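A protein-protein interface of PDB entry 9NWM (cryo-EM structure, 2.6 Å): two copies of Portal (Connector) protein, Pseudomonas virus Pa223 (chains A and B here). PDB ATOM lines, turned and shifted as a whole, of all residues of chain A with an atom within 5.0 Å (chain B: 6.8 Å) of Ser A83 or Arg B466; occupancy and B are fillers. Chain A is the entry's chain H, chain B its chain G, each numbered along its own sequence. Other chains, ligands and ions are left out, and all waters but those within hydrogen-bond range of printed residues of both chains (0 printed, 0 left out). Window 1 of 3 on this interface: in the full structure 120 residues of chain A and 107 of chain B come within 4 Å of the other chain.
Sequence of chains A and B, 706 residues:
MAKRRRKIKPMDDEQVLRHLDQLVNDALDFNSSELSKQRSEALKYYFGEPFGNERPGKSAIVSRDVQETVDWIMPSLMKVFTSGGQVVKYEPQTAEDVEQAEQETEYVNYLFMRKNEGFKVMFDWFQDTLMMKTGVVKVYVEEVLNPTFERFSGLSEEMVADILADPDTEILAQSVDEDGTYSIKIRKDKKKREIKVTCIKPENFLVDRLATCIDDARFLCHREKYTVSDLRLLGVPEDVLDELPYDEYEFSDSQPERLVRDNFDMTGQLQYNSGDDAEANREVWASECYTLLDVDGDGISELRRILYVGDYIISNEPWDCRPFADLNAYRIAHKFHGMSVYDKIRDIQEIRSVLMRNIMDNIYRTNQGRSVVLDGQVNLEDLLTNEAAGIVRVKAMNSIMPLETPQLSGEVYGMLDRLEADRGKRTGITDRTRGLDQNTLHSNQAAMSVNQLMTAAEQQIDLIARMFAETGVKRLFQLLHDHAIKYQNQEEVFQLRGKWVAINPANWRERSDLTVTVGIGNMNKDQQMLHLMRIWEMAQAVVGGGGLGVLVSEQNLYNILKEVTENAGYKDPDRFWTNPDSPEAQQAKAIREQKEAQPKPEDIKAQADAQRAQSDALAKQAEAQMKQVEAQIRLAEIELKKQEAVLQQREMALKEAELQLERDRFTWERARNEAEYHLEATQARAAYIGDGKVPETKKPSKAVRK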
ATOM      1  N   MET A  78      -1.798  17.409   1.955  1.00  0.00           N
ATOM      2  CA  MET A  78      -2.939  18.161   2.465  1.00  0.00           C
ATOM      3  C   MET A  78      -3.559  19.050   1.392  1.00  0.00           C
ATOM      4  O   MET A  78      -4.793  19.114   1.268  1.00  0.00           O
ATOM      5  CB  MET A  78      -2.519  19.005   3.668  1.00  0.00           C
ATOM      6  CG  MET A  78      -2.400  18.220   4.963  1.00  0.00           C
ATOM      7  SD  MET A  78      -3.608  16.894   5.105  1.00  0.00           S
ATOM      8  CE  MET A  78      -4.930  17.729   5.968  1.00  0.00           C
ATOM      9  N   LYS A  79      -2.714  19.730   0.610  1.00  0.00           N
ATOM     10  CA  LYS A  79      -3.206  20.550  -0.491  1.00  0.00           C
ATOM     11  C   LYS A  79      -4.048  19.720  -1.444  1.00  0.00           C
ATOM     12  O   LYS A  79      -5.160  20.112  -1.814  1.00  0.00           O
ATOM     13  CB  LYS A  79      -2.034  21.194  -1.227  1.00  0.00           C
ATOM     14  CG  LYS A  79      -2.447  22.147  -2.328  1.00  0.00           C
ATOM     15  CD  LYS A  79      -1.331  22.338  -3.334  1.00  0.00           C
ATOM     16  CE  LYS A  79      -0.077  22.876  -2.674  1.00  0.00           C
ATOM     17  NZ  LYS A  79       1.149  22.468  -3.412  1.00  0.00           N
ATOM     18  N   PHE A  81      -6.560  16.807  -1.553  1.00  0.00           N
ATOM     19  CA  PHE A  81      -7.613  16.361  -0.636  1.00  0.00           C
ATOM     20  C   PHE A  81      -8.155  17.469   0.262  1.00  0.00           C
ATOM     21  O   PHE A  81      -9.119  17.206   0.985  1.00  0.00           O
ATOM     22  CB  PHE A  81      -7.182  15.216   0.297  1.00  0.00           C
ATOM     23  CG  PHE A  81      -6.691  13.993  -0.411  1.00  0.00           C
ATOM     24  CD1 PHE A  81      -7.545  13.227  -1.178  1.00  0.00           C
ATOM     25  CD2 PHE A  81      -5.372  13.600  -0.295  1.00  0.00           C
ATOM     26  CE1 PHE A  81      -7.090  12.097  -1.820  1.00  0.00           C
ATOM     27  CE2 PHE A  81      -4.912  12.474  -0.936  1.00  0.00           C
ATOM     28  CZ  PHE A  81      -5.772  11.721  -1.700  1.00  0.00           C
ATOM     29  N   THR A  82      -7.601  18.683   0.257  1.00  0.00           N
ATOM     30  CA  THR A  82      -8.179  19.736   1.086  1.00  0.00           C
ATOM     31  C   THR A  82      -8.452  21.052   0.365  1.00  0.00           C
ATOM     32  O   THR A  82      -9.432  21.721   0.713  1.00  0.00           O
ATOM     33  CB  THR A  82      -7.272  20.006   2.296  1.00  0.00           C
ATOM     34  OG1 THR A  82      -7.150  18.807   3.069  1.00  0.00           O
ATOM     35  CG2 THR A  82      -7.850  21.093   3.182  1.00  0.00           C
ATOM     36  N   SER A  83      -7.669  21.416  -0.652  1.00  0.00           N
ATOM     37  CA  SER A  83      -7.654  22.796  -1.136  1.00  0.00           C
ATOM     38  C   SER A  83      -9.024  23.244  -1.633  1.00  0.00           C
ATOM     39  O   SER A  83      -9.401  24.410  -1.476  1.00  0.00           O
ATOM     40  CB  SER A  83      -6.611  22.950  -2.240  1.00  0.00           C
ATOM     41  OG  SER A  83      -6.898  22.092  -3.329  1.00  0.00           O
ATOM     42  N   GLY A  84      -9.784  22.338  -2.234  1.00  0.00           N
ATOM     43  CA  GLY A  84     -11.011  22.739  -2.887  1.00  0.00           C
ATOM     44  C   GLY A  84     -12.183  23.055  -1.988  1.00  0.00           C
ATOM     45  O   GLY A  84     -13.259  23.381  -2.493  1.00  0.00           O
ATOM     46  N   GLY A  85     -12.019  22.978  -0.675  1.00  0.00           N
ATOM     47  CA  GLY A  85     -13.164  23.138   0.221  1.00  0.00           C
ATOM     48  C   GLY A  85     -14.005  21.889   0.328  1.00  0.00           C
ATOM     49  O   GLY A  85     -14.214  21.375   1.430  1.00  0.00           O
ATOM     50  N   PHE A 119     -10.593  18.143   9.000  1.00  0.00           N
ATOM     51  CA  PHE A 119      -9.215  18.480   8.657  1.00  0.00           C
ATOM     52  C   PHE A 119      -8.237  17.891   9.666  1.00  0.00           C
ATOM     53  O   PHE A 119      -7.209  17.317   9.289  1.00  0.00           O
ATOM     54  CB  PHE A 119      -9.054  19.997   8.570  1.00  0.00           C
ATOM     55  CG  PHE A 119      -7.703  20.436   8.090  1.00  0.00           C
ATOM     56  CD1 PHE A 119      -6.672  20.661   8.985  1.00  0.00           C
ATOM     57  CD2 PHE A 119      -7.462  20.625   6.743  1.00  0.00           C
ATOM     58  CE1 PHE A 119      -5.430  21.061   8.544  1.00  0.00           C
ATOM     59  CE2 PHE A 119      -6.221  21.028   6.299  1.00  0.00           C
ATOM     60  CZ  PHE A 119      -5.205  21.246   7.200  1.00  0.00           C
ATOM     61  N   GLN A 438      -1.958  20.839  -7.326  1.00  0.00           N
ATOM     62  CA  GLN A 438      -3.218  20.605  -6.634  1.00  0.00           C
ATOM     63  C   GLN A 438      -4.292  20.004  -7.531  1.00  0.00           C
ATOM     64  O   GLN A 438      -5.448  19.912  -7.107  1.00  0.00           O
ATOM     65  CB  GLN A 438      -3.722  21.910  -6.015  1.00  0.00           C
ATOM     66  CG  GLN A 438      -4.438  22.832  -6.980  1.00  0.00           C
ATOM     67  CD  GLN A 438      -5.293  23.854  -6.268  1.00  0.00           C
ATOM     68  OE1 GLN A 438      -5.072  24.158  -5.097  1.00  0.00           O
ATOM     69  NE2 GLN A 438      -6.278  24.393  -6.972  1.00  0.00           N
ATOM     70  N   ASN A 522     -11.348  19.802  -6.886  1.00  0.00           N
ATOM     71  CA  ASN A 522     -10.682  21.091  -6.991  1.00  0.00           C
ATOM     72  C   ASN A 522     -11.205  21.913  -8.156  1.00  0.00           C
ATOM     73  O   ASN A 522     -12.307  21.676  -8.662  1.00  0.00           O
ATOM     74  CB  ASN A 522      -9.169  20.915  -7.105  1.00  0.00           C
ATOM     75  CG  ASN A 522      -8.524  20.638  -5.770  1.00  0.00           C
ATOM     76  OD1 ASN A 522      -7.970  19.569  -5.545  1.00  0.00           O
ATOM     77  ND2 ASN A 522      -8.597  21.608  -4.871  1.00  0.00           N
ATOM     78  N   LEU B  77       1.908  35.543   7.127  1.00  0.00           N
ATOM     79  CA  LEU B  77       0.735  35.100   7.867  1.00  0.00           C
ATOM     80  C   LEU B  77      -0.211  36.241   8.190  1.00  0.00           C
ATOM     81  O   LEU B  77      -1.367  35.983   8.535  1.00  0.00           O
ATOM     82  CB  LEU B  77       1.155  34.415   9.164  1.00  0.00           C
ATOM     83  CG  LEU B  77       1.643  32.974   9.062  1.00  0.00           C
ATOM     84  CD1 LEU B  77       1.904  32.420  10.448  1.00  0.00           C
ATOM     85  CD2 LEU B  77       0.632  32.124   8.323  1.00  0.00           C
ATOM     86  N   PHE B  81      -5.027  36.689   5.623  1.00  0.00           N
ATOM     87  CA  PHE B  81      -5.991  36.965   6.685  1.00  0.00           C
ATOM     88  C   PHE B  81      -6.154  38.457   6.981  1.00  0.00           C
ATOM     89  O   PHE B  81      -7.009  38.801   7.795  1.00  0.00           O
ATOM     90  CB  PHE B  81      -5.661  36.263   8.018  1.00  0.00           C
ATOM     91  CG  PHE B  81      -5.579  34.771   7.929  1.00  0.00           C
ATOM     92  CD1 PHE B  81      -6.701  34.014   7.660  1.00  0.00           C
ATOM     93  CD2 PHE B  81      -4.375  34.124   8.134  1.00  0.00           C
ATOM     94  CE1 PHE B  81      -6.620  32.640   7.587  1.00  0.00           C
ATOM     95  CE2 PHE B  81      -4.290  32.754   8.061  1.00  0.00           C
ATOM     96  CZ  PHE B  81      -5.413  32.010   7.787  1.00  0.00           C
ATOM     97  N   THR B 440      -3.273  32.741  -1.728  1.00  0.00           N
ATOM     98  CA  THR B 440      -2.920  31.328  -1.654  1.00  0.00           C
ATOM     99  C   THR B 440      -4.135  30.455  -1.369  1.00  0.00           C
ATOM    100  O   THR B 440      -4.278  29.374  -1.952  1.00  0.00           O
ATOM    101  CB  THR B 440      -1.853  31.113  -0.585  1.00  0.00           C
ATOM    102  OG1 THR B 440      -0.826  32.099  -0.729  1.00  0.00           O
ATOM    103  CG2 THR B 440      -1.240  29.731  -0.716  1.00  0.00           C
ATOM    104  N   LEU B 441      -5.017  30.898  -0.481  1.00  0.00           N
ATOM    105  CA  LEU B 441      -6.108  30.064   0.003  1.00  0.00           C
ATOM    106  C   LEU B 441      -7.384  30.196  -0.817  1.00  0.00           C
ATOM    107  O   LEU B 441      -8.391  29.576  -0.463  1.00  0.00           O
ATOM    108  CB  LEU B 441      -6.403  30.392   1.467  1.00  0.00           C
ATOM    109  CG  LEU B 441      -5.304  30.017   2.460  1.00  0.00           C
ATOM    110  CD1 LEU B 441      -5.720  30.370   3.873  1.00  0.00           C
ATOM    111  CD2 LEU B 441      -4.967  28.543   2.352  1.00  0.00           C
ATOM    112  N   HIS B 442      -7.375  30.983  -1.890  1.00  0.00           N
ATOM    113  CA  HIS B 442      -8.580  31.159  -2.689  1.00  0.00           C
ATOM    114  C   HIS B 442      -8.991  29.864  -3.369  1.00  0.00           C
ATOM    115  O   HIS B 442      -8.157  29.145  -3.928  1.00  0.00           O
ATOM    116  CB  HIS B 442      -8.369  32.242  -3.746  1.00  0.00           C
ATOM    117  CG  HIS B 442      -8.426  33.636  -3.211  1.00  0.00           C
ATOM    118  ND1 HIS B 442      -8.963  33.940  -1.979  1.00  0.00           N
ATOM    119  CD2 HIS B 442      -8.031  34.812  -3.750  1.00  0.00           C
ATOM    120  CE1 HIS B 442      -8.888  35.244  -1.779  1.00  0.00           C
ATOM    121  NE2 HIS B 442      -8.324  35.795  -2.837  1.00  0.00           N
ATOM    122  N   SER B 443     -10.286  29.566  -3.314  1.00  0.00           N
ATOM    123  CA  SER B 443     -10.887  28.630  -4.249  1.00  0.00           C
ATOM    124  C   SER B 443     -11.163  29.365  -5.553  1.00  0.00           C
ATOM    125  O   SER B 443     -11.367  30.583  -5.558  1.00  0.00           O
ATOM    126  CB  SER B 443     -12.178  28.045  -3.677  1.00  0.00           C
ATOM    127  OG  SER B 443     -13.172  29.043  -3.539  1.00  0.00           O
ATOM    128  N   ILE B 461       5.673  26.525   4.874  1.00  0.00           N
ATOM    129  CA  ILE B 461       5.010  27.747   5.317  1.00  0.00           C
ATOM    130  C   ILE B 461       3.567  27.764   4.838  1.00  0.00           C
ATOM    131  O   ILE B 461       2.645  28.070   5.605  1.00  0.00           O
ATOM    132  CB  ILE B 461       5.783  28.985   4.830  1.00  0.00           C
ATOM    133  CG1 ILE B 461       7.243  28.906   5.271  1.00  0.00           C
ATOM    134  CG2 ILE B 461       5.139  30.252   5.357  1.00  0.00           C
ATOM    135  CD1 ILE B 461       7.417  28.799   6.763  1.00  0.00           C
ATOM    136  N   ASP B 462       3.349  27.395   3.574  1.00  0.00           N
ATOM    137  CA  ASP B 462       1.997  27.325   3.036  1.00  0.00           C
ATOM    138  C   ASP B 462       1.113  26.450   3.913  1.00  0.00           C
ATOM    139  O   ASP B 462      -0.016  26.826   4.247  1.00  0.00           O
ATOM    140  CB  ASP B 462       2.041  26.790   1.604  1.00  0.00           C
ATOM    141  CG  ASP B 462       0.702  26.881   0.899  1.00  0.00           C
ATOM    142  OD1 ASP B 462      -0.281  27.332   1.519  1.00  0.00           O
ATOM    143  OD2 ASP B 462       0.634  26.492  -0.284  1.00  0.00           O
ATOM    144  N   LEU B 463       1.634  25.293   4.331  1.00  0.00           N
ATOM    145  CA  LEU B 463       0.839  24.393   5.158  1.00  0.00           C
ATOM    146  C   LEU B 463       0.366  25.092   6.422  1.00  0.00           C
ATOM    147  O   LEU B 463      -0.791  24.938   6.827  1.00  0.00           O
ATOM    148  CB  LEU B 463       1.642  23.142   5.503  1.00  0.00           C
ATOM    149  CG  LEU B 463       0.940  22.157   6.437  1.00  0.00           C
ATOM    150  CD1 LEU B 463      -0.359  21.675   5.825  1.00  0.00           C
ATOM    151  CD2 LEU B 463       1.842  20.982   6.757  1.00  0.00           C
ATOM    152  N   ILE B 464       1.236  25.900   7.033  1.00  0.00           N
ATOM    153  CA  ILE B 464       0.836  26.644   8.224  1.00  0.00           C
ATOM    154  C   ILE B 464      -0.387  27.493   7.918  1.00  0.00           C
ATOM    155  O   ILE B 464      -1.397  27.443   8.631  1.00  0.00           O
ATOM    156  CB  ILE B 464       2.002  27.502   8.741  1.00  0.00           C
ATOM    157  CG1 ILE B 464       3.169  26.615   9.170  1.00  0.00           C
ATOM    158  CG2 ILE B 464       1.550  28.372   9.892  1.00  0.00           C
ATOM    159  CD1 ILE B 464       4.460  27.371   9.370  1.00  0.00           C
ATOM    160  N   ALA B 465      -0.336  28.242   6.812  1.00  0.00           N
ATOM    161  CA  ALA B 465      -1.464  29.085   6.443  1.00  0.00           C
ATOM    162  C   ALA B 465      -2.731  28.267   6.264  1.00  0.00           C
ATOM    163  O   ALA B 465      -3.828  28.750   6.559  1.00  0.00           O
ATOM    164  CB  ALA B 465      -1.148  29.862   5.167  1.00  0.00           C
ATOM    165  N   ARG B 466      -2.604  27.027   5.794  1.00  0.00           N
ATOM    166  CA  ARG B 466      -3.781  26.175   5.694  1.00  0.00           C
ATOM    167  C   ARG B 466      -4.242  25.719   7.069  1.00  0.00           C
ATOM    168  O   ARG B 466      -5.437  25.778   7.381  1.00  0.00           O
ATOM    169  CB  ARG B 466      -3.487  24.976   4.796  1.00  0.00           C
ATOM    170  CG  ARG B 466      -4.689  24.480   4.022  1.00  0.00           C
ATOM    171  CD  ARG B 466      -4.291  23.441   2.993  1.00  0.00           C
ATOM    172  NE  ARG B 466      -3.378  23.983   1.996  1.00  0.00           N
ATOM    173  CZ  ARG B 466      -3.756  24.702   0.949  1.00  0.00           C
ATOM    174  NH1 ARG B 466      -5.029  24.983   0.727  1.00  0.00           N
ATOM    175  NH2 ARG B 466      -2.834  25.152   0.103  1.00  0.00           N
ATOM    176  N   MET B 467      -3.303  25.297   7.919  1.00  0.00           N
ATOM    177  CA  MET B 467      -3.678  24.741   9.214  1.00  0.00           C
ATOM    178  C   MET B 467      -4.379  25.780  10.075  1.00  0.00           C
ATOM    179  O   MET B 467      -5.327  25.461  10.801  1.00  0.00           O
ATOM    180  CB  MET B 467      -2.445  24.193   9.926  1.00  0.00           C
ATOM    181  CG  MET B 467      -2.741  23.567  11.272  1.00  0.00           C
ATOM    182  SD  MET B 467      -1.680  22.159  11.623  1.00  0.00           S
ATOM    183  CE  MET B 467      -2.541  20.871  10.731  1.00  0.00           C
ATOM    184  N   PHE B 468      -3.926  27.031  10.007  1.00  0.00           N
ATOM    185  CA  PHE B 468      -4.596  28.100  10.735  1.00  0.00           C
ATOM    186  C   PHE B 468      -6.008  28.318  10.210  1.00  0.00           C
ATOM    187  O   PHE B 468      -6.928  28.613  10.981  1.00  0.00           O
ATOM    188  CB  PHE B 468      -3.789  29.392  10.632  1.00  0.00           C
ATOM    189  CG  PHE B 468      -2.602  29.446  11.549  1.00  0.00           C
ATOM    190  CD1 PHE B 468      -2.190  28.324  12.242  1.00  0.00           C
ATOM    191  CD2 PHE B 468      -1.894  30.619  11.710  1.00  0.00           C
ATOM    192  CE1 PHE B 468      -1.100  28.376  13.081  1.00  0.00           C
ATOM    193  CE2 PHE B 468      -0.803  30.676  12.546  1.00  0.00           C
ATOM    194  CZ  PHE B 468      -0.405  29.552  13.232  1.00  0.00           C
ATOM    195  N   ALA B 469      -6.200  28.178   8.897  1.00  0.00           N
ATOM    196  CA  ALA B 469      -7.485  28.527   8.307  1.00  0.00           C
ATOM    197  C   ALA B 469      -8.554  27.486   8.605  1.00  0.00           C
ATOM    198  O   ALA B 469      -9.732  27.834   8.741  1.00  0.00           O
ATOM    199  CB  ALA B 469      -7.337  28.712   6.799  1.00  0.00           C
ATOM    200  N   GLU B 470      -8.177  26.216   8.709  1.00  0.00           N
ATOM    201  CA  GLU B 470      -9.149  25.142   8.833  1.00  0.00           C
ATOM    202  C   GLU B 470      -9.422  24.722  10.270  1.00  0.00           C
ATOM    203  O   GLU B 470     -10.392  23.996  10.506  1.00  0.00           O
ATOM    204  CB  GLU B 470      -8.687  23.921   8.033  1.00  0.00           C
ATOM    205  CG  GLU B 470      -8.363  24.226   6.585  1.00  0.00           C
ATOM    206  CD  GLU B 470      -9.595  24.273   5.711  1.00  0.00           C
ATOM    207  OE1 GLU B 470     -10.703  24.017   6.227  1.00  0.00           O
ATOM    208  OE2 GLU B 470      -9.459  24.567   4.505  1.00  0.00           O
ATOM    209  N   THR B 471      -8.602  25.146  11.230  1.00  0.00           N
ATOM    210  CA  THR B 471      -8.756  24.690  12.607  1.00  0.00           C
ATOM    211  C   THR B 471      -9.127  25.815  13.562  1.00  0.00           C
ATOM    212  O   THR B 471     -10.152  25.721  14.242  1.00  0.00           O
ATOM    213  CB  THR B 471      -7.470  24.000  13.076  1.00  0.00           C
ATOM    214  OG1 THR B 471      -6.383  24.930  13.024  1.00  0.00           O
ATOM    215  CG2 THR B 471      -7.152  22.812  12.188  1.00  0.00           C
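OD1 of Asp B462 lies within salt-bridge range of NH2 of Arg B466 (3.6 Å). The backbone carbonyl oxygen of Met B467 is in hydrogen-bond range of the side-chain hydroxyl of Thr B471. The backbone carbonyl oxygen of Lys A79 sits at hydrogen-bond distance from the side-chain hydroxyl of Ser A83. The side-chain hydroxyl of Ser A83 is in hydrogen-bond range of the side-chain amide oxygen of Gln A438 (3.3 Å).
Among the printed residues, pairs that only touch across the chains: Phe A119 with Glu B470, Phe A119 with Met B467, Lys A79 with Arg B466, Phe A119 with Thr B471 and Ser A83 with Arg B466.
Of the printed residues of chain B, Lys A79 touches Arg B466. Of the printed residues of chain B, Phe A119 touches Met B467, Glu B470 and Thr B471. Ala B465 touches none of the printed residues of chain A. Of the printed residues of chain A, Glu B470 touches Phe A119 (3.6 Å). Printed residues of chain A within 4 Å of Thr B471: Phe A119. The nearest residue of chain B that does not touch Ser A83 is Ser B443 (5.1 Å). The nearest printed residue of chain B that does not touch Lys A79 is Asp B462 (4.4 Å).
Of the 10 printed residues of chain A, 3 touch a printed residue of chain B. Hydrophobic or aromatic side chains of chain A that line the printed part of chain B: Phe A119. Along chain A the printed residues that touch a printed residue of chain B span positions 79 to 119. Hydrophobic or aromatic side chains of chain B that line the printed part of chain A: Met B467. Among the printed residues, 5 pairs touch across the chains.
Position printed for both chains: 81.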
